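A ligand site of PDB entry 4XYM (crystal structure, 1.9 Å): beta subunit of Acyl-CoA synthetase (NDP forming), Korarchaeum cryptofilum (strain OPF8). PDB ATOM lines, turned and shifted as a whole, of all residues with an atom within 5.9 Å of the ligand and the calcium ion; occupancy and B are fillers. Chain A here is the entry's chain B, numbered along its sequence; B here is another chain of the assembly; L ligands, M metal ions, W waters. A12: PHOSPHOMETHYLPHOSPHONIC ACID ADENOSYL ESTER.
The backbone NH of Ser 70 is in hydrogen-bond range of an oxygen (O1B) of the ligand, 2.9 Å away. The side-chain amino group (NZ) of Lys 60 is in salt-bridge range of an oxygen (O2A) of the ligand (2.8 Å). OG of Ser 70 sits at hydrogen-bond distance from O1B of the ligand, at 3.0 Å. The side-chain amide oxygen (OE1) of Gln 111 lies within hydrogen-bond range of a nitrogen (N6) of the ligand. An oxygen (O2B) of the ligand is in hydrogen-bond range of the backbone NH (N) of Lys 69. NZ of Lys 69 lies within salt-bridge range of O2A of the ligand. N1 of the ligand is in hydrogen-bond range of N of Ala 114. N6 of the ligand is in hydrogen-bond range of O of Glu 112 (3.0 Å).
NZ of Lys 24 sits at hydrogen-bond distance from OG1 of Thr 35. The side-chain amide oxygen (OE1) of Gln 111 sits at hydrogen-bond distance from the side-chain amino group (NZ) of Lys 60. The side-chain amino group (NZ) of Lys 60 lies within salt-bridge range of the side-chain carboxylate (OE2) of Glu 20 (2.9 Å). The side-chain amino group (NZ) of Lys 24 is in hydrogen-bond range of the backbone carbonyl oxygen (O) of Val 223 (2.8 Å). The side-chain amino group (NZ) of Lys 60 sits at hydrogen-bond distance from the backbone carbonyl oxygen (O) of Val 223 (2.8 Å). The side-chain amide nitrogen of Gln 111 lies within hydrogen-bond range of the side-chain carboxylate of Glu 20, 3.0 Å away. NZ of Lys 69 is in salt-bridge range of OE1 of Glu 20. NZ of Lys 24 is in hydrogen-bond range of OE1 of Gln 111, 2.8 Å away.
O2B of the ligand lies close to O of Val 67 (3.2 Å). Thr 35 touches the ligand. CG2 of Val 58 touches C6 of the ligand, 3.7 Å away. His 68 touches the ligand. Val 75 touches the ligand (CG2 to C3A, 3.7 Å). Val 77 touches the ligand (CG1 to N9, 3.96 Å). Phe 113 touches the ligand. Glu 119 touches the ligand (OE2 to O2', 3.6 Å). CD of Pro 212 touches O3' of the ligand (3.3 Å). CG1 of Val 223 touches N7 of the ligand, 3.2 Å away. Hydrophobic or aromatic side chains that line the ligand: Val 58, Val 75, Val 77, Phe 113, Ala 114, Pro 212 and Val 223. Of the 24 residues printed, 18 come within 4 Å of the ligand.
Two residues have an atom within 4 Å of the calcium ion: Asn 211 and Asp 224. The nearest printed residue that does not touch the calcium ion is Pro 212 (4.002 Å).
The backbone carbonyl oxygen (O) of Asn 211 binds the calcium ion (2.3 Å). An oxygen (O3B) of the ligand is bound to the calcium ion (2.3 Å). The calcium ion is bound by O1A of the ligand (2.3 Å). Water W2 binds the calcium ion, at 2.5 Å. Water W7 binds the calcium ion, at 2.5 Å. The calcium ion is bound by OD2 of Asp 224, at 2.5 Å. Water W3 is bound to the calcium ion (2.6 Å). The calcium ion has seven donor atoms within binding distance.
Water W6 lies within hydrogen-bond range of O1B of the ligand, OD1 of Asp 71 and N of Ser 70. Water W5 bridges an oxygen (O2B) of the ligand (2.7 Å) and the backbone carbonyl oxygen of Val 67 (2.9 Å).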
ATOM      1  N   GLU A  20     -33.774   6.648 -25.277  1.00  0.00           N
ATOM      2  CA  GLU A  20     -32.896   6.321 -24.155  1.00  0.00           C
ATOM      3  C   GLU A  20     -32.941   4.844 -23.753  1.00  0.00           C
ATOM      4  O   GLU A  20     -31.888   4.218 -23.588  1.00  0.00           O
ATOM      5  CB  GLU A  20     -33.240   7.199 -22.939  1.00  0.00           C
ATOM      6  CG  GLU A  20     -32.299   6.931 -21.758  1.00  0.00           C
ATOM      7  CD  GLU A  20     -32.599   7.759 -20.518  1.00  0.00           C
ATOM      8  OE1 GLU A  20     -33.411   8.700 -20.606  1.00  0.00           O
ATOM      9  OE2 GLU A  20     -32.020   7.433 -19.452  1.00  0.00           O
ATOM     10  N   LYS A  24     -29.854   2.341 -24.374  1.00  0.00           N
ATOM     11  CA  LYS A  24     -29.229   1.686 -23.241  1.00  0.00           C
ATOM     12  C   LYS A  24     -29.274   0.171 -23.380  1.00  0.00           C
ATOM     13  O   LYS A  24     -28.259  -0.498 -23.151  1.00  0.00           O
ATOM     14  CB  LYS A  24     -29.879   2.128 -21.931  1.00  0.00           C
ATOM     15  CG  LYS A  24     -29.522   3.544 -21.527  1.00  0.00           C
ATOM     16  CD  LYS A  24     -29.965   3.881 -20.126  1.00  0.00           C
ATOM     17  CE  LYS A  24     -29.557   5.296 -19.752  1.00  0.00           C
ATOM     18  NZ  LYS A  24     -30.186   5.745 -18.480  1.00  0.00           N
ATOM     19  N   THR A  35     -27.868   1.895 -16.716  1.00  0.00           N
ATOM     20  CA  THR A  35     -28.801   1.851 -15.599  1.00  0.00           C
ATOM     21  C   THR A  35     -29.866   0.772 -15.827  1.00  0.00           C
ATOM     22  O   THR A  35     -30.304   0.540 -16.947  1.00  0.00           O
ATOM     23  CB  THR A  35     -29.524   3.182 -15.439  1.00  0.00           C
ATOM     24  OG1 THR A  35     -30.310   3.392 -16.615  1.00  0.00           O
ATOM     25  CG2 THR A  35     -28.555   4.339 -15.251  1.00  0.00           C
ATOM     26  N   VAL A  58     -34.815   7.615 -10.584  1.00  0.00           N
ATOM     27  CA  VAL A  58     -34.855   8.747 -11.489  1.00  0.00           C
ATOM     28  C   VAL A  58     -35.968   8.499 -12.492  1.00  0.00           C
ATOM     29  O   VAL A  58     -36.117   7.367 -12.984  1.00  0.00           O
ATOM     30  CB  VAL A  58     -33.513   8.928 -12.217  1.00  0.00           C
ATOM     31  CG1 VAL A  58     -33.623   9.996 -13.293  1.00  0.00           C
ATOM     32  CG2 VAL A  58     -32.417   9.258 -11.232  1.00  0.00           C
ATOM     33  N   LYS A  60     -37.665  10.026 -16.210  1.00  0.00           N
ATOM     34  CA  LYS A  60     -37.387  10.821 -17.398  1.00  0.00           C
ATOM     35  C   LYS A  60     -38.485  10.652 -18.451  1.00  0.00           C
ATOM     36  O   LYS A  60     -39.028   9.563 -18.631  1.00  0.00           O
ATOM     37  CB  LYS A  60     -36.049  10.430 -18.023  1.00  0.00           C
ATOM     38  CG  LYS A  60     -34.842  10.558 -17.115  1.00  0.00           C
ATOM     39  CD  LYS A  60     -33.587  10.125 -17.868  1.00  0.00           C
ATOM     40  CE  LYS A  60     -32.357  10.116 -16.979  1.00  0.00           C
ATOM     41  NZ  LYS A  60     -31.182   9.549 -17.692  1.00  0.00           N
ATOM     42  N   VAL A  67     -35.344  15.632 -27.339  1.00  0.00           N
ATOM     43  CA  VAL A  67     -33.976  15.146 -27.321  1.00  0.00           C
ATOM     44  C   VAL A  67     -33.267  15.679 -26.073  1.00  0.00           C
ATOM     45  O   VAL A  67     -32.541  14.944 -25.404  1.00  0.00           O
ATOM     46  CB  VAL A  67     -33.199  15.543 -28.605  1.00  0.00           C
ATOM     47  CG1 VAL A  67     -33.203  17.048 -28.801  1.00  0.00           C
ATOM     48  CG2 VAL A  67     -31.766  14.987 -28.554  1.00  0.00           C
ATOM     49  N   HIS A  68     -33.487  16.955 -25.770  1.00  0.00           N
ATOM     50  CA  HIS A  68     -32.904  17.575 -24.574  1.00  0.00           C
ATOM     51  C   HIS A  68     -33.954  17.591 -23.460  1.00  0.00           C
ATOM     52  O   HIS A  68     -34.796  18.477 -23.384  1.00  0.00           O
ATOM     53  CB  HIS A  68     -32.416  18.999 -24.884  1.00  0.00           C
ATOM     54  CG  HIS A  68     -31.513  19.081 -26.077  1.00  0.00           C
ATOM     55  ND1 HIS A  68     -30.233  18.569 -26.084  1.00  0.00           N
ATOM     56  CD2 HIS A  68     -31.704  19.626 -27.308  1.00  0.00           C
ATOM     57  CE1 HIS A  68     -29.684  18.780 -27.266  1.00  0.00           C
ATOM     58  NE2 HIS A  68     -30.559  19.413 -28.033  1.00  0.00           N
ATOM     59  N   LYS A  69     -33.875  16.606 -22.574  1.00  0.00           N
ATOM     60  CA  LYS A  69     -34.937  16.358 -21.608  1.00  0.00           C
ATOM     61  C   LYS A  69     -34.907  17.336 -20.433  1.00  0.00           C
ATOM     62  O   LYS A  69     -35.944  17.789 -19.986  1.00  0.00           O
ATOM     63  CB  LYS A  69     -34.836  14.915 -21.139  1.00  0.00           C
ATOM     64  CG  LYS A  69     -35.116  13.911 -22.282  1.00  0.00           C
ATOM     65  CD  LYS A  69     -34.733  12.490 -21.935  1.00  0.00           C
ATOM     66  CE  LYS A  69     -33.235  12.384 -22.023  1.00  0.00           C
ATOM     67  NZ  LYS A  69     -32.606  11.419 -21.135  1.00  0.00           N
ATOM     68  N   SER A  70     -33.714  17.649 -19.924  1.00  0.00           N
ATOM     69  CA  SER A  70     -33.598  18.592 -18.813  1.00  0.00           C
ATOM     70  C   SER A  70     -34.129  19.983 -19.186  1.00  0.00           C
ATOM     71  O   SER A  70     -34.811  20.625 -18.404  1.00  0.00           O
ATOM     72  CB  SER A  70     -32.147  18.724 -18.364  1.00  0.00           C
ATOM     73  OG  SER A  70     -31.674  17.496 -17.888  1.00  0.00           O
ATOM     74  N   ASP A  71     -33.810  20.431 -20.401  1.00  0.00           N
ATOM     75  CA  ASP A  71     -34.165  21.784 -20.827  1.00  0.00           C
ATOM     76  C   ASP A  71     -35.673  22.028 -20.801  1.00  0.00           C
ATOM     77  O   ASP A  71     -36.098  23.179 -20.680  1.00  0.00           O
ATOM     78  CB  ASP A  71     -33.633  22.045 -22.245  1.00  0.00           C
ATOM     79  CG  ASP A  71     -32.128  22.188 -22.289  1.00  0.00           C
ATOM     80  OD1 ASP A  71     -31.480  22.222 -21.212  1.00  0.00           O
ATOM     81  OD2 ASP A  71     -31.578  22.268 -23.408  1.00  0.00           O
ATOM     82  N   VAL A  75     -36.726  15.664 -16.578  1.00  0.00           N
ATOM     83  CA  VAL A  75     -35.863  14.802 -15.772  1.00  0.00           C
ATOM     84  C   VAL A  75     -35.944  15.108 -14.277  1.00  0.00           C
ATOM     85  O   VAL A  75     -35.692  16.230 -13.866  1.00  0.00           O
ATOM     86  CB  VAL A  75     -34.392  14.901 -16.196  1.00  0.00           C
ATOM     87  CG1 VAL A  75     -33.496  13.996 -15.345  1.00  0.00           C
ATOM     88  CG2 VAL A  75     -34.246  14.537 -17.667  1.00  0.00           C
ATOM     89  N   VAL A  77     -34.542  13.599 -10.522  1.00  0.00           N
ATOM     90  CA  VAL A  77     -33.588  12.690  -9.903  1.00  0.00           C
ATOM     91  C   VAL A  77     -33.841  12.544  -8.403  1.00  0.00           C
ATOM     92  O   VAL A  77     -34.579  13.319  -7.815  1.00  0.00           O
ATOM     93  CB  VAL A  77     -32.125  13.145 -10.116  1.00  0.00           C
ATOM     94  CG1 VAL A  77     -31.805  13.227 -11.624  1.00  0.00           C
ATOM     95  CG2 VAL A  77     -31.858  14.463  -9.425  1.00  0.00           C
ATOM     96  N   GLN A 111     -35.512   4.565 -13.662  1.00  0.00           N
ATOM     97  CA  GLN A 111     -34.178   3.991 -13.615  1.00  0.00           C
ATOM     98  C   GLN A 111     -33.537   4.231 -12.268  1.00  0.00           C
ATOM     99  O   GLN A 111     -33.900   5.166 -11.561  1.00  0.00           O
ATOM    100  CB  GLN A 111     -33.301   4.567 -14.732  1.00  0.00           C
ATOM    101  CG  GLN A 111     -33.040   6.062 -14.672  1.00  0.00           C
ATOM    102  CD  GLN A 111     -32.587   6.630 -16.009  1.00  0.00           C
ATOM    103  OE1 GLN A 111     -31.402   6.831 -16.253  1.00  0.00           O
ATOM    104  NE2 GLN A 111     -33.557   6.894 -16.889  1.00  0.00           N
ATOM    105  N   GLU A 112     -32.561   3.392 -11.932  1.00  0.00           N
ATOM    106  CA  GLU A 112     -31.838   3.541 -10.686  1.00  0.00           C
ATOM    107  C   GLU A 112     -31.196   4.919 -10.626  1.00  0.00           C
ATOM    108  O   GLU A 112     -30.917   5.529 -11.648  1.00  0.00           O
ATOM    109  CB  GLU A 112     -30.793   2.439 -10.526  1.00  0.00           C
ATOM    110  CG  GLU A 112     -29.622   2.572 -11.466  1.00  0.00           C
ATOM    111  CD  GLU A 112     -28.945   1.234 -11.759  1.00  0.00           C
ATOM    112  OE1 GLU A 112     -29.666   0.231 -11.940  1.00  0.00           O
ATOM    113  OE2 GLU A 112     -27.694   1.191 -11.802  1.00  0.00           O
ATOM    114  N   PHE A 113     -30.994   5.411  -9.414  1.00  0.00           N
ATOM    115  CA  PHE A 113     -30.295   6.659  -9.189  1.00  0.00           C
ATOM    116  C   PHE A 113     -28.812   6.397  -9.026  1.00  0.00           C
ATOM    117  O   PHE A 113     -28.420   5.715  -8.073  1.00  0.00           O
ATOM    118  CB  PHE A 113     -30.837   7.385  -7.958  1.00  0.00           C
ATOM    119  CG  PHE A 113     -30.061   8.612  -7.593  1.00  0.00           C
ATOM    120  CD1 PHE A 113     -30.094   9.741  -8.397  1.00  0.00           C
ATOM    121  CD2 PHE A 113     -29.296   8.645  -6.434  1.00  0.00           C
ATOM    122  CE1 PHE A 113     -29.380  10.886  -8.065  1.00  0.00           C
ATOM    123  CE2 PHE A 113     -28.581   9.788  -6.092  1.00  0.00           C
ATOM    124  CZ  PHE A 113     -28.624  10.908  -6.907  1.00  0.00           C
ATOM    125  N   ALA A 114     -28.009   6.853  -9.978  1.00  0.00           N
ATOM    126  CA  ALA A 114     -26.581   6.674  -9.876  1.00  0.00           C
ATOM    127  C   ALA A 114     -26.008   7.731  -8.922  1.00  0.00           C
ATOM    128  O   ALA A 114     -26.276   8.915  -9.087  1.00  0.00           O
ATOM    129  CB  ALA A 114     -25.945   6.766 -11.245  1.00  0.00           C
ATOM    130  N   PRO A 115     -25.229   7.311  -7.916  1.00  0.00           N
ATOM    131  CA  PRO A 115     -24.681   8.318  -6.990  1.00  0.00           C
ATOM    132  C   PRO A 115     -23.578   9.148  -7.663  1.00  0.00           C
ATOM    133  O   PRO A 115     -23.027   8.708  -8.673  1.00  0.00           O
ATOM    134  CB  PRO A 115     -24.133   7.491  -5.832  1.00  0.00           C
ATOM    135  CG  PRO A 115     -23.995   6.086  -6.356  1.00  0.00           C
ATOM    136  CD  PRO A 115     -25.024   5.936  -7.435  1.00  0.00           C
ATOM    137  N   GLU A 119     -17.956  12.502 -13.893  1.00  0.00           N
ATOM    138  CA  GLU A 119     -18.733  12.398 -15.133  1.00  0.00           C
ATOM    139  C   GLU A 119     -17.813  12.405 -16.357  1.00  0.00           C
ATOM    140  O   GLU A 119     -16.842  13.159 -16.417  1.00  0.00           O
ATOM    141  CB  GLU A 119     -19.743  13.546 -15.235  1.00  0.00           C
ATOM    142  CG  GLU A 119     -20.909  13.451 -14.270  1.00  0.00           C
ATOM    143  CD  GLU A 119     -22.054  14.390 -14.637  1.00  0.00           C
ATOM    144  OE1 GLU A 119     -21.927  15.135 -15.632  1.00  0.00           O
ATOM    145  OE2 GLU A 119     -23.079  14.393 -13.928  1.00  0.00           O
ATOM    146  N   ASN A 211     -23.678  10.644 -22.593  1.00  0.00           N
ATOM    147  CA  ASN A 211     -23.416  11.885 -21.862  1.00  0.00           C
ATOM    148  C   ASN A 211     -24.483  12.131 -20.807  1.00  0.00           C
ATOM    149  O   ASN A 211     -25.576  12.574 -21.140  1.00  0.00           O
ATOM    150  CB  ASN A 211     -23.369  13.073 -22.818  1.00  0.00           C
ATOM    151  CG  ASN A 211     -23.052  14.382 -22.097  1.00  0.00           C
ATOM    152  OD1 ASN A 211     -22.931  14.407 -20.859  1.00  0.00           O
ATOM    153  ND2 ASN A 211     -22.932  15.457 -22.845  1.00  0.00           N
ATOM    154  N   PRO A 212     -24.167  11.864 -19.526  1.00  0.00           N
ATOM    155  CA  PRO A 212     -22.891  11.426 -18.957  1.00  0.00           C
ATOM    156  C   PRO A 212     -22.803   9.951 -18.634  1.00  0.00           C
ATOM    157  O   PRO A 212     -23.800   9.232 -18.478  1.00  0.00           O
ATOM    158  CB  PRO A 212     -22.828  12.219 -17.666  1.00  0.00           C
ATOM    159  CG  PRO A 212     -24.216  12.190 -17.190  1.00  0.00           C
ATOM    160  CD  PRO A 212     -25.106  12.241 -18.451  1.00  0.00           C
ATOM    161  N   ILE A 214     -21.029   7.983 -15.571  1.00  0.00           N
ATOM    162  CA  ILE A 214     -20.469   8.250 -14.252  1.00  0.00           C
ATOM    163  C   ILE A 214     -19.404   7.194 -13.903  1.00  0.00           C
ATOM    164  O   ILE A 214     -19.659   5.982 -13.953  1.00  0.00           O
ATOM    165  CB  ILE A 214     -21.571   8.310 -13.193  1.00  0.00           C
ATOM    166  CG1 ILE A 214     -22.600   9.343 -13.656  1.00  0.00           C
ATOM    167  CG2 ILE A 214     -20.981   8.676 -11.840  1.00  0.00           C
ATOM    168  CD1 ILE A 214     -23.628   9.719 -12.633  1.00  0.00           C
ATOM    169  N   VAL A 223     -25.492   6.742 -17.843  1.00  0.00           N
ATOM    170  CA  VAL A 223     -26.693   7.302 -17.242  1.00  0.00           C
ATOM    171  C   VAL A 223     -27.630   7.937 -18.293  1.00  0.00           C
ATOM    172  O   VAL A 223     -28.827   8.109 -18.049  1.00  0.00           O
ATOM    173  CB  VAL A 223     -26.260   8.295 -16.139  1.00  0.00           C
ATOM    174  CG1 VAL A 223     -27.012   9.585 -16.217  1.00  0.00           C
ATOM    175  CG2 VAL A 223     -26.395   7.632 -14.779  1.00  0.00           C
ATOM    176  N   ASP A 224     -27.087   8.325 -19.441  1.00  0.00           N
ATOM    177  CA  ASP A 224     -27.895   8.781 -20.574  1.00  0.00           C
ATOM    178  C   ASP A 224     -27.279   8.262 -21.866  1.00  0.00           C
ATOM    179  O   ASP A 224     -26.066   8.080 -21.950  1.00  0.00           O
ATOM    180  CB  ASP A 224     -28.016  10.304 -20.609  1.00  0.00           C
ATOM    181  CG  ASP A 224     -28.991  10.809 -21.688  1.00  0.00           C
ATOM    182  OD1 ASP A 224     -29.821  10.011 -22.187  1.00  0.00           O
ATOM    183  OD2 ASP A 224     -28.925  12.016 -22.025  1.00  0.00           O
ATOM    184  N   ARG B 178     -23.540  26.954 -19.718  1.00  0.00           N
ATOM    185  CA  ARG B 178     -24.777  26.265 -19.351  1.00  0.00           C
ATOM    186  C   ARG B 178     -25.183  26.506 -17.892  1.00  0.00           C
ATOM    187  O   ARG B 178     -24.511  26.065 -16.961  1.00  0.00           O
ATOM    188  CB  ARG B 178     -24.639  24.762 -19.606  1.00  0.00           C
ATOM    189  CG  ARG B 178     -25.702  23.920 -18.893  1.00  0.00           C
ATOM    190  CD  ARG B 178     -25.958  22.578 -19.557  1.00  0.00           C
ATOM    191  NE  ARG B 178     -27.173  22.628 -20.360  1.00  0.00           N
ATOM    192  CZ  ARG B 178     -27.707  21.604 -21.006  1.00  0.00           C
ATOM    193  NH1 ARG B 178     -27.143  20.402 -20.959  1.00  0.00           N
ATOM    194  NH2 ARG B 178     -28.816  21.781 -21.708  1.00  0.00           N
HETATM  195  PB  A12 L   1     -30.669  15.375 -21.140  1.00  0.00           P
HETATM  196  O1B A12 L   1     -31.086  16.798 -20.710  1.00  0.00           O
HETATM  197  O2B A12 L   1     -31.525  14.902 -22.332  1.00  0.00           O
HETATM  198  O3B A12 L   1     -29.213  15.267 -21.462  1.00  0.00           O
HETATM  199  PA  A12 L   1     -30.023  13.318 -18.999  1.00  0.00           P
HETATM  200  O1A A12 L   1     -28.547  13.330 -19.364  1.00  0.00           O
HETATM  201  O2A A12 L   1     -30.588  11.872 -19.097  1.00  0.00           O
HETATM  202  C3A A12 L   1     -31.228  14.397 -19.761  1.00  0.00           C
HETATM  203  O5' A12 L   1     -30.256  13.753 -17.510  1.00  0.00           O
HETATM  204  C5' A12 L   1     -29.871  15.064 -17.060  1.00  0.00           C
HETATM  205  C4' A12 L   1     -28.889  14.919 -15.931  1.00  0.00           C
HETATM  206  O4' A12 L   1     -29.521  14.292 -14.797  1.00  0.00           O
HETATM  207  C3' A12 L   1     -27.671  14.053 -16.199  1.00  0.00           C
HETATM  208  O3' A12 L   1     -26.656  14.760 -16.921  1.00  0.00           O
HETATM  209  C2' A12 L   1     -27.233  13.717 -14.784  1.00  0.00           C
HETATM  210  O2' A12 L   1     -26.615  14.834 -14.164  1.00  0.00           O
HETATM  211  C1' A12 L   1     -28.595  13.454 -14.128  1.00  0.00           C
HETATM  212  N9  A12 L   1     -29.046  12.077 -14.215  1.00  0.00           N
HETATM  213  C8  A12 L   1     -29.696  11.484 -15.278  1.00  0.00           C
HETATM  214  N7  A12 L   1     -29.910  10.197 -15.126  1.00  0.00           N
HETATM  215  C5  A12 L   1     -29.382   9.924 -13.882  1.00  0.00           C
HETATM  216  C6  A12 L   1     -29.271   8.729 -13.145  1.00  0.00           C
HETATM  217  N6  A12 L   1     -29.708   7.553 -13.578  1.00  0.00           N
HETATM  218  N1  A12 L   1     -28.670   8.792 -11.935  1.00  0.00           N
HETATM  219  C2  A12 L   1     -28.212   9.971 -11.511  1.00  0.00           C
HETATM  220  N3  A12 L   1     -28.247  11.165 -12.115  1.00  0.00           N
HETATM  221  C4  A12 L   1     -28.846  11.069 -13.300  1.00  0.00           C
HETATM  222 CA    CA M   1     -27.402  13.887 -21.285  1.00  0.00          CA
HETATM  223  O   HOH W   1     -27.738  13.341 -10.271  1.00  0.00           O
HETATM  224  O   HOH W   2     -27.448  13.525 -23.719  1.00  0.00           O
HETATM  225  O   HOH W   3     -26.101  15.737 -22.471  1.00  0.00           O
HETATM  226  O   HOH W   4     -29.221  17.019 -23.916  1.00  0.00           O
HETATM  227  O   HOH W   5     -30.056  13.835 -24.380  1.00  0.00           O
HETATM  228  O   HOH W   6     -31.210  19.071 -21.782  1.00  0.00           O
HETATM  229  O   HOH W   7     -26.424  15.445 -19.569  1.00  0.00           O
